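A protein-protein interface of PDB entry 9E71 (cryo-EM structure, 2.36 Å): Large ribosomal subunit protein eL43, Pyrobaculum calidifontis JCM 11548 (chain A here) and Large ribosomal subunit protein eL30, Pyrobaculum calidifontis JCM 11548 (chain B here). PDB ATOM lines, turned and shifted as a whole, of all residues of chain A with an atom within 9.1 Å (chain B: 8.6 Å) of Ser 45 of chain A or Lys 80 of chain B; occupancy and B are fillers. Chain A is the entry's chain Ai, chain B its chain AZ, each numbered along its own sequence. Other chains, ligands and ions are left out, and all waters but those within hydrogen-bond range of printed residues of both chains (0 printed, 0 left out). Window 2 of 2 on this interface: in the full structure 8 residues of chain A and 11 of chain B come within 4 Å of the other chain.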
ATOM      1  N   LYS A  37     -22.437 -15.734  22.165  1.00  0.00           N
ATOM      2  CA  LYS A  37     -21.964 -14.978  21.018  1.00  0.00           C
ATOM      3  C   LYS A  37     -22.768 -15.353  19.783  1.00  0.00           C
ATOM      4  O   LYS A  37     -23.114 -16.518  19.584  1.00  0.00           O
ATOM      5  CB  LYS A  37     -20.478 -15.236  20.777  1.00  0.00           C
ATOM      6  CG  LYS A  37     -19.580 -14.144  21.321  1.00  0.00           C
ATOM      7  CD  LYS A  37     -18.404 -14.729  22.074  1.00  0.00           C
ATOM      8  CE  LYS A  37     -17.521 -13.630  22.639  1.00  0.00           C
ATOM      9  NZ  LYS A  37     -16.072 -13.920  22.453  1.00  0.00           N
ATOM     10  N   HIS A  38     -23.068 -14.359  18.952  1.00  0.00           N
ATOM     11  CA  HIS A  38     -23.850 -14.571  17.749  1.00  0.00           C
ATOM     12  C   HIS A  38     -23.113 -14.006  16.546  1.00  0.00           C
ATOM     13  O   HIS A  38     -22.276 -13.109  16.663  1.00  0.00           O
ATOM     14  CB  HIS A  38     -25.238 -13.926  17.856  1.00  0.00           C
ATOM     15  CG  HIS A  38     -25.884 -14.097  19.194  1.00  0.00           C
ATOM     16  ND1 HIS A  38     -25.724 -13.194  20.222  1.00  0.00           N
ATOM     17  CD2 HIS A  38     -26.684 -15.077  19.676  1.00  0.00           C
ATOM     18  CE1 HIS A  38     -26.402 -13.606  21.277  1.00  0.00           C
ATOM     19  NE2 HIS A  38     -26.993 -14.747  20.973  1.00  0.00           N
ATOM     20  N   ARG A  39     -23.436 -14.553  15.381  1.00  0.00           N
ATOM     21  CA  ARG A  39     -22.964 -14.028  14.108  1.00  0.00           C
ATOM     22  C   ARG A  39     -23.851 -12.854  13.724  1.00  0.00           C
ATOM     23  O   ARG A  39     -25.072 -13.006  13.629  1.00  0.00           O
ATOM     24  CB  ARG A  39     -23.015 -15.108  13.027  1.00  0.00           C
ATOM     25  CG  ARG A  39     -21.761 -15.259  12.185  1.00  0.00           C
ATOM     26  CD  ARG A  39     -20.696 -16.090  12.885  1.00  0.00           C
ATOM     27  NE  ARG A  39     -19.678 -16.554  11.950  1.00  0.00           N
ATOM     28  CZ  ARG A  39     -18.379 -16.608  12.214  1.00  0.00           C
ATOM     29  NH1 ARG A  39     -17.900 -16.239  13.390  1.00  0.00           N
ATOM     30  NH2 ARG A  39     -17.542 -17.039  11.275  1.00  0.00           N
ATOM     31  N   CYS A  40     -23.246 -11.693  13.518  1.00  0.00           N
ATOM     32  CA  CYS A  40     -24.015 -10.530  13.101  1.00  0.00           C
ATOM     33  C   CYS A  40     -24.581 -10.763  11.703  1.00  0.00           C
ATOM     34  O   CYS A  40     -23.868 -11.253  10.820  1.00  0.00           O
ATOM     35  CB  CYS A  40     -23.151  -9.269  13.114  1.00  0.00           C
ATOM     36  SG  CYS A  40     -23.901  -7.838  12.300  1.00  0.00           S
ATOM     37  N   PRO A  41     -25.854 -10.439  11.468  1.00  0.00           N
ATOM     38  CA  PRO A  41     -26.440 -10.690  10.143  1.00  0.00           C
ATOM     39  C   PRO A  41     -25.825  -9.858   9.041  1.00  0.00           C
ATOM     40  O   PRO A  41     -25.914 -10.247   7.872  1.00  0.00           O
ATOM     41  CB  PRO A  41     -27.924 -10.344  10.335  1.00  0.00           C
ATOM     42  CG  PRO A  41     -28.098 -10.025  11.782  1.00  0.00           C
ATOM     43  CD  PRO A  41     -26.768  -9.689  12.338  1.00  0.00           C
ATOM     44  N   SER A  42     -25.199  -8.730   9.374  1.00  0.00           N
ATOM     45  CA  SER A  42     -24.602  -7.855   8.374  1.00  0.00           C
ATOM     46  C   SER A  42     -23.131  -8.183   8.144  1.00  0.00           C
ATOM     47  O   SER A  42     -22.742  -8.571   7.040  1.00  0.00           O
ATOM     48  CB  SER A  42     -24.759  -6.396   8.809  1.00  0.00           C
ATOM     49  OG  SER A  42     -24.704  -5.523   7.699  1.00  0.00           O
ATOM     50  N   CYS A  43     -22.309  -8.050   9.179  1.00  0.00           N
ATOM     51  CA  CYS A  43     -20.870  -8.221   9.041  1.00  0.00           C
ATOM     52  C   CYS A  43     -20.414  -9.648   9.301  1.00  0.00           C
ATOM     53  O   CYS A  43     -19.240  -9.954   9.084  1.00  0.00           O
ATOM     54  CB  CYS A  43     -20.128  -7.261   9.977  1.00  0.00           C
ATOM     55  SG  CYS A  43     -20.222  -7.655  11.735  1.00  0.00           S
ATOM     56  N   ARG A  44     -21.306 -10.524   9.759  1.00  0.00           N
ATOM     57  CA  ARG A  44     -21.023 -11.943   9.972  1.00  0.00           C
ATOM     58  C   ARG A  44     -19.942 -12.182  11.018  1.00  0.00           C
ATOM     59  O   ARG A  44     -19.323 -13.247  11.041  1.00  0.00           O
ATOM     60  CB  ARG A  44     -20.641 -12.634   8.662  1.00  0.00           C
ATOM     61  CG  ARG A  44     -21.456 -12.188   7.477  1.00  0.00           C
ATOM     62  CD  ARG A  44     -22.231 -13.332   6.892  1.00  0.00           C
ATOM     63  NE  ARG A  44     -23.353 -12.861   6.094  1.00  0.00           N
ATOM     64  CZ  ARG A  44     -24.039 -13.618   5.252  1.00  0.00           C
ATOM     65  NH1 ARG A  44     -23.740 -14.892   5.069  1.00  0.00           N
ATOM     66  NH2 ARG A  44     -25.049 -13.082   4.575  1.00  0.00           N
ATOM     67  N   SER A  45     -19.706 -11.214  11.894  1.00  0.00           N
ATOM     68  CA  SER A  45     -18.719 -11.387  12.946  1.00  0.00           C
ATOM     69  C   SER A  45     -19.321 -12.147  14.115  1.00  0.00           C
ATOM     70  O   SER A  45     -20.508 -12.011  14.419  1.00  0.00           O
ATOM     71  CB  SER A  45     -18.201 -10.031  13.422  1.00  0.00           C
ATOM     72  OG  SER A  45     -17.393  -9.421  12.441  1.00  0.00           O
ATOM     73  N   LEU A  46     -18.494 -12.963  14.760  1.00  0.00           N
ATOM     74  CA  LEU A  46     -18.856 -13.611  16.015  1.00  0.00           C
ATOM     75  C   LEU A  46     -18.651 -12.572  17.105  1.00  0.00           C
ATOM     76  O   LEU A  46     -17.523 -12.302  17.521  1.00  0.00           O
ATOM     77  CB  LEU A  46     -18.013 -14.865  16.225  1.00  0.00           C
ATOM     78  CG  LEU A  46     -18.114 -15.840  17.407  1.00  0.00           C
ATOM     79  CD1 LEU A  46     -17.777 -15.235  18.765  1.00  0.00           C
ATOM     80  CD2 LEU A  46     -19.508 -16.439  17.423  1.00  0.00           C
ATOM     81  N   VAL A  47     -19.744 -11.968  17.561  1.00  0.00           N
ATOM     82  CA  VAL A  47     -19.701 -10.861  18.502  1.00  0.00           C
ATOM     83  C   VAL A  47     -20.827 -11.076  19.509  1.00  0.00           C
ATOM     84  O   VAL A  47     -21.817 -11.749  19.227  1.00  0.00           O
ATOM     85  CB  VAL A  47     -19.824  -9.502  17.768  1.00  0.00           C
ATOM     86  CG1 VAL A  47     -20.974  -9.528  16.786  1.00  0.00           C
ATOM     87  CG2 VAL A  47     -19.927  -8.311  18.709  1.00  0.00           C
ATOM     88  N   ARG A  48     -20.646 -10.543  20.715  1.00  0.00           N
ATOM     89  CA  ARG A  48     -21.727 -10.490  21.696  1.00  0.00           C
ATOM     90  C   ARG A  48     -22.607  -9.300  21.340  1.00  0.00           C
ATOM     91  O   ARG A  48     -22.297  -8.158  21.682  1.00  0.00           O
ATOM     92  CB  ARG A  48     -21.178 -10.375  23.114  1.00  0.00           C
ATOM     93  CG  ARG A  48     -22.254 -10.318  24.190  1.00  0.00           C
ATOM     94  CD  ARG A  48     -21.730  -9.740  25.501  1.00  0.00           C
ATOM     95  NE  ARG A  48     -22.818  -9.355  26.394  1.00  0.00           N
ATOM     96  CZ  ARG A  48     -22.718  -9.274  27.714  1.00  0.00           C
ATOM     97  NH1 ARG A  48     -21.576  -9.512  28.338  1.00  0.00           N
ATOM     98  NH2 ARG A  48     -23.792  -8.942  28.426  1.00  0.00           N
ATOM     99  N   LEU A  49     -23.704  -9.564  20.639  1.00  0.00           N
ATOM    100  CA  LEU A  49     -24.624  -8.504  20.262  1.00  0.00           C
ATOM    101  C   LEU A  49     -25.311  -7.925  21.493  1.00  0.00           C
ATOM    102  O   LEU A  49     -25.544  -8.615  22.486  1.00  0.00           O
ATOM    103  CB  LEU A  49     -25.668  -9.035  19.282  1.00  0.00           C
ATOM    104  CG  LEU A  49     -25.136  -9.586  17.963  1.00  0.00           C
ATOM    105  CD1 LEU A  49     -26.240 -10.259  17.183  1.00  0.00           C
ATOM    106  CD2 LEU A  49     -24.512  -8.490  17.141  1.00  0.00           C
ATOM    107  N   CYS A  59     -25.195  -4.665  16.698  1.00  0.00           N
ATOM    108  CA  CYS A  59     -23.827  -5.149  16.554  1.00  0.00           C
ATOM    109  C   CYS A  59     -22.847  -4.044  16.915  1.00  0.00           C
ATOM    110  O   CYS A  59     -22.890  -2.971  16.302  1.00  0.00           O
ATOM    111  CB  CYS A  59     -23.563  -5.618  15.137  1.00  0.00           C
ATOM    112  SG  CYS A  59     -21.837  -6.078  14.830  1.00  0.00           S
ATOM    113  N   PRO A  60     -21.953  -4.257  17.884  1.00  0.00           N
ATOM    114  CA  PRO A  60     -20.964  -3.225  18.218  1.00  0.00           C
ATOM    115  C   PRO A  60     -19.858  -3.068  17.190  1.00  0.00           C
ATOM    116  O   PRO A  60     -19.173  -2.036  17.200  1.00  0.00           O
ATOM    117  CB  PRO A  60     -20.399  -3.704  19.558  1.00  0.00           C
ATOM    118  CG  PRO A  60     -20.649  -5.161  19.591  1.00  0.00           C
ATOM    119  CD  PRO A  60     -21.751  -5.499  18.641  1.00  0.00           C
ATOM    120  N   LYS A  61     -19.663  -4.039  16.300  1.00  0.00           N
ATOM    121  CA  LYS A  61     -18.610  -3.938  15.296  1.00  0.00           C
ATOM    122  C   LYS A  61     -19.007  -3.006  14.156  1.00  0.00           C
ATOM    123  O   LYS A  61     -18.377  -1.966  13.950  1.00  0.00           O
ATOM    124  CB  LYS A  61     -18.265  -5.328  14.755  1.00  0.00           C
ATOM    125  CG  LYS A  61     -17.999  -6.359  15.828  1.00  0.00           C
ATOM    126  CD  LYS A  61     -16.519  -6.495  16.099  1.00  0.00           C
ATOM    127  CE  LYS A  61     -16.245  -6.719  17.570  1.00  0.00           C
ATOM    128  NZ  LYS A  61     -14.818  -7.039  17.820  1.00  0.00           N
ATOM    129  N   CYS A  62     -20.055  -3.358  13.416  1.00  0.00           N
ATOM    130  CA  CYS A  62     -20.458  -2.600  12.243  1.00  0.00           C
ATOM    131  C   CYS A  62     -21.608  -1.640  12.505  1.00  0.00           C
ATOM    132  O   CYS A  62     -22.008  -0.917  11.588  1.00  0.00           O
ATOM    133  CB  CYS A  62     -20.842  -3.553  11.107  1.00  0.00           C
ATOM    134  SG  CYS A  62     -22.363  -4.467  11.391  1.00  0.00           S
ATOM    135  N   ILE B  19      -4.237  -4.279   0.117  1.00  0.00           N
ATOM    136  CA  ILE B  19      -5.253  -4.827   1.007  1.00  0.00           C
ATOM    137  C   ILE B  19      -5.852  -3.698   1.830  1.00  0.00           C
ATOM    138  O   ILE B  19      -5.124  -2.863   2.378  1.00  0.00           O
ATOM    139  CB  ILE B  19      -4.666  -5.920   1.915  1.00  0.00           C
ATOM    140  CG1 ILE B  19      -4.338  -7.165   1.091  1.00  0.00           C
ATOM    141  CG2 ILE B  19      -5.625  -6.260   3.037  1.00  0.00           C
ATOM    142  CD1 ILE B  19      -3.527  -8.188   1.836  1.00  0.00           C
ATOM    143  N   GLY B  20      -7.176  -3.672   1.915  1.00  0.00           N
ATOM    144  CA  GLY B  20      -7.860  -2.682   2.718  1.00  0.00           C
ATOM    145  C   GLY B  20      -8.725  -1.760   1.890  1.00  0.00           C
ATOM    146  O   GLY B  20      -8.377  -1.432   0.755  1.00  0.00           O
ATOM    147  N   LEU B  21      -9.859  -1.336   2.451  1.00  0.00           N
ATOM    148  CA  LEU B  21     -10.788  -0.497   1.701  1.00  0.00           C
ATOM    149  C   LEU B  21     -10.200   0.880   1.425  1.00  0.00           C
ATOM    150  O   LEU B  21     -10.351   1.413   0.322  1.00  0.00           O
ATOM    151  CB  LEU B  21     -12.110  -0.380   2.457  1.00  0.00           C
ATOM    152  CG  LEU B  21     -13.306   0.194   1.697  1.00  0.00           C
ATOM    153  CD1 LEU B  21     -13.417   1.690   1.923  1.00  0.00           C
ATOM    154  CD2 LEU B  21     -13.194  -0.113   0.219  1.00  0.00           C
ATOM    155  N   ALA B  39     -15.827  -7.673  -1.233  1.00  0.00           N
ATOM    156  CA  ALA B  39     -16.546  -8.735  -0.546  1.00  0.00           C
ATOM    157  C   ALA B  39     -18.046  -8.608  -0.784  1.00  0.00           C
ATOM    158  O   ALA B  39     -18.585  -7.508  -0.931  1.00  0.00           O
ATOM    159  CB  ALA B  39     -16.248  -8.707   0.950  1.00  0.00           C
ATOM    160  N   ASN B  41     -20.554  -9.221   1.189  1.00  0.00           N
ATOM    161  CA  ASN B  41     -21.291  -8.641   2.303  1.00  0.00           C
ATOM    162  C   ASN B  41     -20.799  -7.244   2.654  1.00  0.00           C
ATOM    163  O   ASN B  41     -20.977  -6.791   3.789  1.00  0.00           O
ATOM    164  CB  ASN B  41     -21.216  -9.555   3.525  1.00  0.00           C
ATOM    165  CG  ASN B  41     -19.849  -9.550   4.169  1.00  0.00           C
ATOM    166  OD1 ASN B  41     -18.833  -9.393   3.497  1.00  0.00           O
ATOM    167  ND2 ASN B  41     -19.817  -9.719   5.483  1.00  0.00           N
ATOM    168  N   PRO B  43     -20.701  -3.235   2.998  1.00  0.00           N
ATOM    169  CA  PRO B  43     -21.807  -2.319   3.278  1.00  0.00           C
ATOM    170  C   PRO B  43     -22.156  -1.485   2.060  1.00  0.00           C
ATOM    171  O   PRO B  43     -21.411  -1.405   1.082  1.00  0.00           O
ATOM    172  CB  PRO B  43     -21.289  -1.442   4.423  1.00  0.00           C
ATOM    173  CG  PRO B  43     -19.915  -1.873   4.707  1.00  0.00           C
ATOM    174  CD  PRO B  43     -19.478  -2.900   3.732  1.00  0.00           C
ATOM    175  N   SER B  67     -17.884 -13.484   2.253  1.00  0.00           N
ATOM    176  CA  SER B  67     -17.939 -12.293   3.079  1.00  0.00           C
ATOM    177  C   SER B  67     -16.545 -11.699   3.238  1.00  0.00           C
ATOM    178  O   SER B  67     -15.569 -12.173   2.654  1.00  0.00           O
ATOM    179  CB  SER B  67     -18.550 -12.623   4.437  1.00  0.00           C
ATOM    180  OG  SER B  67     -17.668 -13.416   5.210  1.00  0.00           O
ATOM    181  N   SER B  68     -16.453 -10.641   4.049  1.00  0.00           N
ATOM    182  CA  SER B  68     -15.159 -10.044   4.359  1.00  0.00           C
ATOM    183  C   SER B  68     -14.254 -11.035   5.080  1.00  0.00           C
ATOM    184  O   SER B  68     -13.050 -11.109   4.799  1.00  0.00           O
ATOM    185  CB  SER B  68     -15.360  -8.796   5.212  1.00  0.00           C
ATOM    186  OG  SER B  68     -15.468  -7.640   4.408  1.00  0.00           O
ATOM    187  N   ILE B  69     -14.823 -11.811   6.004  1.00  0.00           N
ATOM    188  CA  ILE B  69     -14.034 -12.767   6.772  1.00  0.00           C
ATOM    189  C   ILE B  69     -13.475 -13.854   5.868  1.00  0.00           C
ATOM    190  O   ILE B  69     -12.288 -14.186   5.939  1.00  0.00           O
ATOM    191  CB  ILE B  69     -14.878 -13.365   7.909  1.00  0.00           C
ATOM    192  CG1 ILE B  69     -15.883 -12.340   8.424  1.00  0.00           C
ATOM    193  CG2 ILE B  69     -13.985 -13.843   9.028  1.00  0.00           C
ATOM    194  CD1 ILE B  69     -15.596 -11.865   9.819  1.00  0.00           C
ATOM    195  N   GLU B  70     -14.311 -14.416   4.993  1.00  0.00           N
ATOM    196  CA  GLU B  70     -13.821 -15.476   4.122  1.00  0.00           C
ATOM    197  C   GLU B  70     -12.913 -14.939   3.027  1.00  0.00           C
ATOM    198  O   GLU B  70     -12.035 -15.663   2.554  1.00  0.00           O
ATOM    199  CB  GLU B  70     -14.982 -16.278   3.534  1.00  0.00           C
ATOM    200  CG  GLU B  70     -16.157 -16.438   4.484  1.00  0.00           C
ATOM    201  CD  GLU B  70     -17.481 -16.596   3.768  1.00  0.00           C
ATOM    202  OE1 GLU B  70     -17.486 -16.556   2.528  1.00  0.00           O
ATOM    203  OE2 GLU B  70     -18.514 -16.774   4.441  1.00  0.00           O
ATOM    204  N   LEU B  71     -13.083 -13.680   2.623  1.00  0.00           N
ATOM    205  CA  LEU B  71     -12.103 -13.074   1.729  1.00  0.00           C
ATOM    206  C   LEU B  71     -10.740 -12.975   2.400  1.00  0.00           C
ATOM    207  O   LEU B  71      -9.713 -13.311   1.794  1.00  0.00           O
ATOM    208  CB  LEU B  71     -12.577 -11.697   1.277  1.00  0.00           C
ATOM    209  CG  LEU B  71     -11.608 -10.943   0.368  1.00  0.00           C
ATOM    210  CD1 LEU B  71     -11.170 -11.825  -0.783  1.00  0.00           C
ATOM    211  CD2 LEU B  71     -12.237  -9.658  -0.146  1.00  0.00           C
ATOM    212  N   GLY B  72     -10.713 -12.532   3.659  1.00  0.00           N
ATOM    213  CA  GLY B  72      -9.455 -12.488   4.387  1.00  0.00           C
ATOM    214  C   GLY B  72      -8.859 -13.865   4.601  1.00  0.00           C
ATOM    215  O   GLY B  72      -7.640 -14.041   4.558  1.00  0.00           O
ATOM    216  N   ALA B  73      -9.713 -14.860   4.830  1.00  0.00           N
ATOM    217  CA  ALA B  73      -9.237 -16.230   4.978  1.00  0.00           C
ATOM    218  C   ALA B  73      -8.643 -16.757   3.678  1.00  0.00           C
ATOM    219  O   ALA B  73      -7.610 -17.435   3.689  1.00  0.00           O
ATOM    220  CB  ALA B  73     -10.376 -17.127   5.454  1.00  0.00           C
ATOM    221  N   ALA B  75      -7.278 -14.934   1.400  1.00  0.00           N
ATOM    222  CA  ALA B  75      -5.998 -14.246   1.304  1.00  0.00           C
ATOM    223  C   ALA B  75      -5.011 -14.680   2.381  1.00  0.00           C
ATOM    224  O   ALA B  75      -3.856 -14.250   2.341  1.00  0.00           O
ATOM    225  CB  ALA B  75      -6.209 -12.734   1.377  1.00  0.00           C
ATOM    226  N   ARG B  77      -5.001 -13.797   5.455  1.00  0.00           N
ATOM    227  CA  ARG B  77      -4.841 -12.821   6.499  1.00  0.00           C
ATOM    228  C   ARG B  77      -5.771 -13.189   7.644  1.00  0.00           C
ATOM    229  O   ARG B  77      -6.914 -13.594   7.397  1.00  0.00           O
ATOM    230  CB  ARG B  77      -5.150 -11.416   5.993  1.00  0.00           C
ATOM    231  CG  ARG B  77      -4.367 -11.035   4.759  1.00  0.00           C
ATOM    232  CD  ARG B  77      -2.889 -10.960   5.072  1.00  0.00           C
ATOM    233  NE  ARG B  77      -2.638 -10.270   6.330  1.00  0.00           N
ATOM    234  CZ  ARG B  77      -1.541  -9.578   6.599  1.00  0.00           C
ATOM    235  NH1 ARG B  77      -0.555  -9.479   5.723  1.00  0.00           N
ATOM    236  NH2 ARG B  77      -1.426  -8.977   7.777  1.00  0.00           N
ATOM    237  N   PRO B  78      -5.343 -13.042   8.898  1.00  0.00           N
ATOM    238  CA  PRO B  78      -6.185 -13.468  10.024  1.00  0.00           C
ATOM    239  C   PRO B  78      -7.275 -12.468  10.380  1.00  0.00           C
ATOM    240  O   PRO B  78      -7.967 -12.625  11.389  1.00  0.00           O
ATOM    241  CB  PRO B  78      -5.182 -13.620  11.177  1.00  0.00           C
ATOM    242  CG  PRO B  78      -3.825 -13.319  10.600  1.00  0.00           C
ATOM    243  CD  PRO B  78      -4.031 -12.558   9.345  1.00  0.00           C
ATOM    244  N   HIS B  79      -7.432 -11.438   9.558  1.00  0.00           N
ATOM    245  CA  HIS B  79      -8.389 -10.370   9.754  1.00  0.00           C
ATOM    246  C   HIS B  79      -9.368 -10.356   8.591  1.00  0.00           C
ATOM    247  O   HIS B  79      -9.379 -11.249   7.744  1.00  0.00           O
ATOM    248  CB  HIS B  79      -7.674  -9.028   9.863  1.00  0.00           C
ATOM    249  CG  HIS B  79      -6.684  -8.796   8.768  1.00  0.00           C
ATOM    250  ND1 HIS B  79      -7.044  -8.303   7.533  1.00  0.00           N
ATOM    251  CD2 HIS B  79      -5.351  -9.012   8.713  1.00  0.00           C
ATOM    252  CE1 HIS B  79      -5.970  -8.207   6.771  1.00  0.00           C
ATOM    253  NE2 HIS B  79      -4.929  -8.625   7.465  1.00  0.00           N
ATOM    254  N   LYS B  80     -10.194  -9.319   8.559  1.00  0.00           N
ATOM    255  CA  LYS B  80     -11.206  -9.171   7.533  1.00  0.00           C
ATOM    256  C   LYS B  80     -10.694  -8.284   6.402  1.00  0.00           C
ATOM    257  O   LYS B  80      -9.731  -7.530   6.556  1.00  0.00           O
ATOM    258  CB  LYS B  80     -12.476  -8.593   8.147  1.00  0.00           C
ATOM    259  CG  LYS B  80     -13.255  -9.591   8.984  1.00  0.00           C
ATOM    260  CD  LYS B  80     -14.031  -8.977  10.165  1.00  0.00           C
ATOM    261  CE  LYS B  80     -14.992  -7.843   9.812  1.00  0.00           C
ATOM    262  NZ  LYS B  80     -14.343  -6.530   9.551  1.00  0.00           N
ATOM    263  N   ILE B  81     -11.343  -8.392   5.245  1.00  0.00           N
ATOM    264  CA  ILE B  81     -10.970  -7.613   4.071  1.00  0.00           C
ATOM    265  C   ILE B  81     -12.238  -7.230   3.324  1.00  0.00           C
ATOM    266  O   ILE B  81     -12.882  -8.092   2.719  1.00  0.00           O
ATOM    267  CB  ILE B  81     -10.022  -8.380   3.143  1.00  0.00           C
ATOM    268  CG1 ILE B  81      -8.647  -8.541   3.784  1.00  0.00           C
ATOM    269  CG2 ILE B  81      -9.905  -7.676   1.813  1.00  0.00           C
ATOM    270  CD1 ILE B  81      -7.730  -9.422   2.991  1.00  0.00           C
ATOM    271  N   MET B  82     -12.595  -5.944   3.349  1.00  0.00           N
ATOM    272  CA  MET B  82     -13.684  -5.491   2.489  1.00  0.00           C
ATOM    273  C   MET B  82     -13.321  -5.601   1.019  1.00  0.00           C
ATOM    274  O   MET B  82     -14.082  -6.177   0.235  1.00  0.00           O
ATOM    275  CB  MET B  82     -14.062  -4.042   2.776  1.00  0.00           C
ATOM    276  CG  MET B  82     -15.522  -3.738   2.485  1.00  0.00           C
ATOM    277  SD  MET B  82     -16.167  -2.324   3.374  1.00  0.00           S
ATOM    278  CE  MET B  82     -15.001  -2.238   4.699  1.00  0.00           C
ATOM    279  N   ALA B  83     -12.176  -5.054   0.627  1.00  0.00           N
ATOM    280  CA  ALA B  83     -11.823  -4.987  -0.780  1.00  0.00           C
ATOM    281  C   ALA B  83     -10.312  -4.975  -0.921  1.00  0.00           C
ATOM    282  O   ALA B  83      -9.594  -4.488  -0.048  1.00  0.00           O
ATOM    283  CB  ALA B  83     -12.422  -3.747  -1.449  1.00  0.00           C
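The side-chain amide oxygen (OD1) of Asn 41 of chain B sits at hydrogen-bond distance from the backbone NH (N) of Ser 68 of chain B (2.7 Å). SG of Cys 40 of chain A lies close to N of Ser 42 of chain A (3.3 Å). NE of Arg 39 of chain A sits close to O of Arg 44 of chain A. The side-chain sulfur (SG) of Cys 43 of chain A lies close to the side-chain hydroxyl (OG) of Ser 45 of chain A, 3.4 Å away. N of Cys 40 of chain A sits at hydrogen-bond distance from O of Ser 45 of chain A.
Among the printed residues, merely in contact across the chains: Ser 42 of chain A with Asn 41 of chain B, Cys 43 of chain A with Asn 41 of chain B, Arg 44 of chain A with Asn 41 of chain B and Ser 45 of chain A with Lys 80 of chain B.
Printed residues of chain B within 4 Å of Ser 42 of chain A: Asn 41. Printed residues of chain B within 4 Å of Cys 43 of chain A: Asn 41. Printed residues of chain B within 4 Å of Arg 44 of chain A: Asn 41. Printed residues of chain B within 4 Å of Ser 45 of chain A: Lys 80. Of the printed residues of chain A, Asn 41 of chain B touches Ser 42, Cys 43 and Arg 44. Ser 68 of chain B touches none of the printed residues of chain A. Of chain A, only Ser 45 (3.9 Å) comes within 4 Å of Lys 80 of chain B. The nearest residue of chain A that does not touch Lys 80 of chain B is Cys 43 of chain A (4.8 Å). The nearest printed residue of chain B that does not touch Cys 43 of chain A is Ile 69 of chain B (4.2 Å).
Of the 21 printed residues of chain B, 2 touch a printed residue of chain A. Of the 17 printed residues of chain A, 4 touch a printed residue of chain B. Among the printed residues, 4 pairs touch across the chains. Among the printed residues, no Asp or Glu carboxylate lies within 4 Å of a Lys or Arg side-chain nitrogen of the other chain.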
